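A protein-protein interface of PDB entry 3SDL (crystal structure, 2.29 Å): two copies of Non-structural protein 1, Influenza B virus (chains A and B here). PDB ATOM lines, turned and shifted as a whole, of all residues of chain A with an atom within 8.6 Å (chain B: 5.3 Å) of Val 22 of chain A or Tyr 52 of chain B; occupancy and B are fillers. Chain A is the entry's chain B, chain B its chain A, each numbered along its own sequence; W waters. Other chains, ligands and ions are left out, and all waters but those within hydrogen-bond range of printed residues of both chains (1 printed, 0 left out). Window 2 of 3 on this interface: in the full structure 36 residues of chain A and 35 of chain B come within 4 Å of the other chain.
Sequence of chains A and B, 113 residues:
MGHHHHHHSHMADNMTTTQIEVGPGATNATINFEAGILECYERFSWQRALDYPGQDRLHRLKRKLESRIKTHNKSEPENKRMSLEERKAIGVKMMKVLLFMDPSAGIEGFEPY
CG of Arg 48 of chain B touches CG2 of Ile 20 of chain A, at 3.7 Å.
Glu 21 of chain A touches Arg 48 of chain B (O to CB, 3.9 Å).
Leu 50 of chain B touches Val 22 of chain A.
Asp 51 of chain B touches Val 22 of chain A (CA to CG1, 3.9 Å).
CG2 of Val 22 of chain A touches CE1 of Tyr 52 of chain B (3.5 Å).
Val 22 of chain A touches Gln 55 of chain B (CG1 to NE2, 3.2 Å).
CB of Ala 26 of chain A touches N of Asp 51 of chain B, at 3.8 Å.
OD2 of Asp 51 of chain B touches CA of Thr 27 of chain A, at 3.8 Å.
Leu 50 of chain B touches Thr 30 of chain A (CA to OG1, 3.4 Å).
O of Leu 50 of chain B sits at hydrogen-bond distance from NE2 of Gln 55 of chain B.
The backbone carbonyl oxygen of Ala 26 of chain A lies within hydrogen-bond range of the side-chain hydroxyl of Thr 30 of chain A (3.0 Å).
N of Gly 54 of chain B lies within hydrogen-bond range of OD1 of Asp 51 of chain B, 2.8 Å away.
Hydrophobic or aromatic side chains of chain B within 4 Å of the printed part of chain A: Leu 50 and Tyr 52.
Of the 11 printed residues of chain A, 6 touch a printed residue of chain B.
Hydrophobic or aromatic side chains of chain A that line the printed part of chain B: Ile 20, Val 22 and Ala 26.
Among the printed residues, 12 pairs touch across the chains.
The backbone carbonyl oxygen (O) of Val 22 of chain A sits close to the backbone carbonyl oxygen (O) of Arg 48 of chain B (3.2 Å).
N of Asp 51 of chain B sits at hydrogen-bond distance from OG1 of Thr 30 of chain A, 3.0 Å away.
O of Ile 20 of chain A lies within hydrogen-bond range of NE2 of Gln 55 of chain B (2.9 Å).
Gln 19 of chain A touches none of the printed residues of chain B.
Of the printed residues of chain B, Ile 20 of chain A touches Arg 48 and Gln 55.
Val 22 of chain A touches five residues of chain B.
Of the printed residues of chain B, Ala 26 of chain A touches Asp 51.
Of the printed residues of chain A, Leu 50 of chain B touches Val 22 (2.9 Å) and Thr 30 (3.4 Å).
Printed residues of chain A within 4 Å of Asp 51 of chain B: Val 22 (3.9 Å), Ala 26 (3.8 Å), Thr 27 (3.8 Å) and Thr 30 (3.0 Å).
Of chain A, only Val 22 comes within 4 Å of Tyr 52 of chain B.
No residue of chain A comes within 4 Å of Pro 53 of chain B.
Gly 54 of chain B touches none of the printed residues of chain A.
Water W1 lies within hydrogen-bond range of the side-chain carboxylate (OD2) of Asp 51 of chain B and the backbone carbonyl oxygen (O) of Thr 27 of chain A.
No position is printed for both chains.
Of the 12 pairs that touch across the chains among the printed residues, none has its exchanged pair printed and touching as well.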
ATOM      1  N   GLN A  19     -17.375  15.811  -6.606  1.00  0.00           N
ATOM      2  CA  GLN A  19     -17.167  17.241  -6.813  1.00  0.00           C
ATOM      3  C   GLN A  19     -15.830  17.724  -6.255  1.00  0.00           C
ATOM      4  O   GLN A  19     -15.157  17.008  -5.512  1.00  0.00           O
ATOM      5  CB  GLN A  19     -18.317  18.050  -6.205  1.00  0.00           C
ATOM      6  CG  GLN A  19     -19.642  17.928  -6.950  1.00  0.00           C
ATOM      7  CD  GLN A  19     -20.284  16.559  -6.800  1.00  0.00           C
ATOM      8  OE1 GLN A  19     -19.939  15.793  -5.900  1.00  0.00           O
ATOM      9  NE2 GLN A  19     -21.225  16.246  -7.685  1.00  0.00           N
ATOM     10  N   ILE A  20     -15.454  18.945  -6.623  1.00  0.00           N
ATOM     11  CA  ILE A  20     -14.206  19.544  -6.166  1.00  0.00           C
ATOM     12  C   ILE A  20     -14.445  20.937  -5.596  1.00  0.00           C
ATOM     13  O   ILE A  20     -14.922  21.827  -6.299  1.00  0.00           O
ATOM     14  CB  ILE A  20     -13.181  19.665  -7.310  1.00  0.00           C
ATOM     15  CG1 ILE A  20     -12.828  18.288  -7.876  1.00  0.00           C
ATOM     16  CG2 ILE A  20     -11.932  20.382  -6.828  1.00  0.00           C
ATOM     17  CD1 ILE A  20     -13.816  17.776  -8.901  1.00  0.00           C
ATOM     18  N   GLU A  21     -14.117  21.125  -4.321  1.00  0.00           N
ATOM     19  CA  GLU A  21     -14.196  22.447  -3.711  1.00  0.00           C
ATOM     20  C   GLU A  21     -13.261  23.383  -4.471  1.00  0.00           C
ATOM     21  O   GLU A  21     -12.117  23.030  -4.756  1.00  0.00           O
ATOM     22  CB  GLU A  21     -13.827  22.388  -2.228  1.00  0.00           C
ATOM     23  CG  GLU A  21     -14.086  23.678  -1.466  1.00  0.00           C
ATOM     24  CD  GLU A  21     -13.913  23.509   0.031  1.00  0.00           C
ATOM     25  OE1 GLU A  21     -13.785  24.533   0.734  1.00  0.00           O
ATOM     26  OE2 GLU A  21     -13.909  22.353   0.506  1.00  0.00           O
ATOM     27  N   VAL A  22     -13.747  24.574  -4.798  1.00  0.00           N
ATOM     28  CA  VAL A  22     -13.054  25.431  -5.755  1.00  0.00           C
ATOM     29  C   VAL A  22     -12.254  26.583  -5.144  1.00  0.00           C
ATOM     30  O   VAL A  22     -11.024  26.593  -5.208  1.00  0.00           O
ATOM     31  CB  VAL A  22     -14.037  25.980  -6.813  1.00  0.00           C
ATOM     32  CG1 VAL A  22     -14.618  24.838  -7.616  1.00  0.00           C
ATOM     33  CG2 VAL A  22     -15.153  26.775  -6.157  1.00  0.00           C
ATOM     34  N   GLY A  23     -12.955  27.549  -4.559  1.00  0.00           N
ATOM     35  CA  GLY A  23     -12.330  28.767  -4.078  1.00  0.00           C
ATOM     36  C   GLY A  23     -12.771  29.965  -4.900  1.00  0.00           C
ATOM     37  O   GLY A  23     -13.149  29.815  -6.062  1.00  0.00           O
ATOM     38  N   PRO A  24     -12.725  31.165  -4.301  1.00  0.00           N
ATOM     39  CA  PRO A  24     -13.206  32.404  -4.926  1.00  0.00           C
ATOM     40  C   PRO A  24     -12.592  32.676  -6.300  1.00  0.00           C
ATOM     41  O   PRO A  24     -13.291  33.137  -7.203  1.00  0.00           O
ATOM     42  CB  PRO A  24     -12.768  33.484  -3.933  1.00  0.00           C
ATOM     43  CG  PRO A  24     -12.692  32.779  -2.623  1.00  0.00           C
ATOM     44  CD  PRO A  24     -12.200  31.400  -2.945  1.00  0.00           C
ATOM     45  N   GLY A  25     -11.303  32.389  -6.450  1.00  0.00           N
ATOM     46  CA  GLY A  25     -10.583  32.698  -7.673  1.00  0.00           C
ATOM     47  C   GLY A  25     -10.896  31.787  -8.846  1.00  0.00           C
ATOM     48  O   GLY A  25     -10.344  31.958  -9.933  1.00  0.00           O
ATOM     49  N   ALA A  26     -11.781  30.819  -8.630  1.00  0.00           N
ATOM     50  CA  ALA A  26     -12.141  29.868  -9.676  1.00  0.00           C
ATOM     51  C   ALA A  26     -12.900  30.558 -10.804  1.00  0.00           C
ATOM     52  O   ALA A  26     -12.739  30.219 -11.978  1.00  0.00           O
ATOM     53  CB  ALA A  26     -12.963  28.730  -9.099  1.00  0.00           C
ATOM     54  N   THR A  27     -13.726  31.533 -10.438  1.00  0.00           N
ATOM     55  CA  THR A  27     -14.539  32.253 -11.405  1.00  0.00           C
ATOM     56  C   THR A  27     -13.682  32.821 -12.530  1.00  0.00           C
ATOM     57  O   THR A  27     -13.936  32.568 -13.706  1.00  0.00           O
ATOM     58  CB  THR A  27     -15.319  33.399 -10.738  1.00  0.00           C
ATOM     59  OG1 THR A  27     -16.026  32.899  -9.596  1.00  0.00           O
ATOM     60  CG2 THR A  27     -16.307  34.007 -11.723  1.00  0.00           C
ATOM     61  N   ALA A  29     -10.551  32.063 -13.201  1.00  0.00           N
ATOM     62  CA  ALA A  29      -9.778  30.987 -13.813  1.00  0.00           C
ATOM     63  C   ALA A  29     -10.579  30.265 -14.890  1.00  0.00           C
ATOM     64  O   ALA A  29     -10.052  29.935 -15.954  1.00  0.00           O
ATOM     65  CB  ALA A  29      -9.307  30.005 -12.753  1.00  0.00           C
ATOM     66  N   THR A  30     -11.857  30.027 -14.610  1.00  0.00           N
ATOM     67  CA  THR A  30     -12.730  29.327 -15.544  1.00  0.00           C
ATOM     68  C   THR A  30     -13.040  30.175 -16.778  1.00  0.00           C
ATOM     69  O   THR A  30     -13.097  29.656 -17.893  1.00  0.00           O
ATOM     70  CB  THR A  30     -14.045  28.890 -14.868  1.00  0.00           C
ATOM     71  OG1 THR A  30     -13.750  28.033 -13.756  1.00  0.00           O
ATOM     72  CG2 THR A  30     -14.934  28.146 -15.853  1.00  0.00           C
ATOM     73  N   ARG B  48      -8.400  22.618  -9.305  1.00  0.00           N
ATOM     74  CA  ARG B  48      -9.385  23.244  -8.432  1.00  0.00           C
ATOM     75  C   ARG B  48      -9.647  24.686  -8.849  1.00  0.00           C
ATOM     76  O   ARG B  48      -9.835  25.568  -8.008  1.00  0.00           O
ATOM     77  CB  ARG B  48      -8.909  23.189  -6.985  1.00  0.00           C
ATOM     78  CG  ARG B  48      -8.487  21.803  -6.551  1.00  0.00           C
ATOM     79  CD  ARG B  48      -7.906  21.814  -5.160  1.00  0.00           C
ATOM     80  NE  ARG B  48      -7.508  20.477  -4.733  1.00  0.00           N
ATOM     81  CZ  ARG B  48      -7.040  20.195  -3.522  1.00  0.00           C
ATOM     82  NH1 ARG B  48      -6.914  21.163  -2.623  1.00  0.00           N
ATOM     83  NH2 ARG B  48      -6.702  18.950  -3.207  1.00  0.00           N
ATOM     84  N   LEU B  50     -11.869  25.132 -11.556  1.00  0.00           N
ATOM     85  CA  LEU B  50     -13.134  25.028 -12.271  1.00  0.00           C
ATOM     86  C   LEU B  50     -14.308  25.310 -11.339  1.00  0.00           C
ATOM     87  O   LEU B  50     -14.634  24.488 -10.484  1.00  0.00           O
ATOM     88  CB  LEU B  50     -13.281  23.636 -12.891  1.00  0.00           C
ATOM     89  CG  LEU B  50     -14.393  23.491 -13.931  1.00  0.00           C
ATOM     90  CD1 LEU B  50     -14.168  24.491 -15.053  1.00  0.00           C
ATOM     91  CD2 LEU B  50     -14.472  22.073 -14.485  1.00  0.00           C
ATOM     92  N   ASP B  51     -14.940  26.469 -11.506  1.00  0.00           N
ATOM     93  CA  ASP B  51     -16.070  26.844 -10.658  1.00  0.00           C
ATOM     94  C   ASP B  51     -17.236  25.876 -10.827  1.00  0.00           C
ATOM     95  O   ASP B  51     -17.203  25.001 -11.691  1.00  0.00           O
ATOM     96  CB  ASP B  51     -16.514  28.286 -10.922  1.00  0.00           C
ATOM     97  CG  ASP B  51     -16.908  28.526 -12.368  1.00  0.00           C
ATOM     98  OD1 ASP B  51     -17.039  27.545 -13.130  1.00  0.00           O
ATOM     99  OD2 ASP B  51     -17.094  29.704 -12.740  1.00  0.00           O
ATOM    100  N   TYR B  52     -18.262  26.029  -9.996  1.00  0.00           N
ATOM    101  CA  TYR B  52     -19.370  25.076  -9.971  1.00  0.00           C
ATOM    102  C   TYR B  52     -20.178  25.045 -11.272  1.00  0.00           C
ATOM    103  O   TYR B  52     -20.462  23.968 -11.797  1.00  0.00           O
ATOM    104  CB  TYR B  52     -20.269  25.318  -8.756  1.00  0.00           C
ATOM    105  CG  TYR B  52     -19.512  25.279  -7.448  1.00  0.00           C
ATOM    106  CD1 TYR B  52     -19.267  26.443  -6.731  1.00  0.00           C
ATOM    107  CD2 TYR B  52     -19.023  24.083  -6.939  1.00  0.00           C
ATOM    108  CE1 TYR B  52     -18.569  26.415  -5.538  1.00  0.00           C
ATOM    109  CE2 TYR B  52     -18.323  24.045  -5.746  1.00  0.00           C
ATOM    110  CZ  TYR B  52     -18.099  25.215  -5.049  1.00  0.00           C
ATOM    111  OH  TYR B  52     -17.403  25.187  -3.862  1.00  0.00           O
ATOM    112  N   PRO B  53     -20.545  26.222 -11.801  1.00  0.00           N
ATOM    113  CA  PRO B  53     -21.217  26.235 -13.103  1.00  0.00           C
ATOM    114  C   PRO B  53     -20.355  25.548 -14.157  1.00  0.00           C
ATOM    115  O   PRO B  53     -20.879  24.826 -15.005  1.00  0.00           O
ATOM    116  CB  PRO B  53     -21.338  27.729 -13.418  1.00  0.00           C
ATOM    117  CG  PRO B  53     -21.336  28.393 -12.086  1.00  0.00           C
ATOM    118  CD  PRO B  53     -20.406  27.576 -11.237  1.00  0.00           C
ATOM    119  N   GLY B  54     -19.045  25.771 -14.090  1.00  0.00           N
ATOM    120  CA  GLY B  54     -18.111  25.181 -15.034  1.00  0.00           C
ATOM    121  C   GLY B  54     -17.993  23.676 -14.891  1.00  0.00           C
ATOM    122  O   GLY B  54     -17.740  22.968 -15.865  1.00  0.00           O
ATOM    123  N   GLN B  55     -18.170  23.186 -13.669  1.00  0.00           N
ATOM    124  CA  GLN B  55     -18.109  21.752 -13.416  1.00  0.00           C
ATOM    125  C   GLN B  55     -19.318  21.045 -14.026  1.00  0.00           C
ATOM    126  O   GLN B  55     -19.224  19.892 -14.448  1.00  0.00           O
ATOM    127  CB  GLN B  55     -18.026  21.467 -11.916  1.00  0.00           C
ATOM    128  CG  GLN B  55     -16.702  21.851 -11.274  1.00  0.00           C
ATOM    129  CD  GLN B  55     -16.684  21.590  -9.773  1.00  0.00           C
ATOM    130  OE1 GLN B  55     -17.477  20.799  -9.258  1.00  0.00           O
ATOM    131  NE2 GLN B  55     -15.782  22.262  -9.066  1.00  0.00           N
ATOM    132  N   ASP B  56     -20.448  21.744 -14.074  1.00  0.00           N
ATOM    133  CA  ASP B  56     -21.655  21.195 -14.682  1.00  0.00           C
ATOM    134  C   ASP B  56     -21.483  21.040 -16.186  1.00  0.00           C
ATOM    135  O   ASP B  56     -21.875  20.027 -16.762  1.00  0.00           O
ATOM    136  CB  ASP B  56     -22.864  22.076 -14.377  1.00  0.00           C
ATOM    137  CG  ASP B  56     -23.348  21.919 -12.952  1.00  0.00           C
ATOM    138  OD1 ASP B  56     -22.916  22.706 -12.084  1.00  0.00           O
ATOM    139  OD2 ASP B  56     -24.155  21.000 -12.700  1.00  0.00           O
HETATM  140  O   HOH W   1     -16.612  31.446 -14.544  1.00  0.00           O
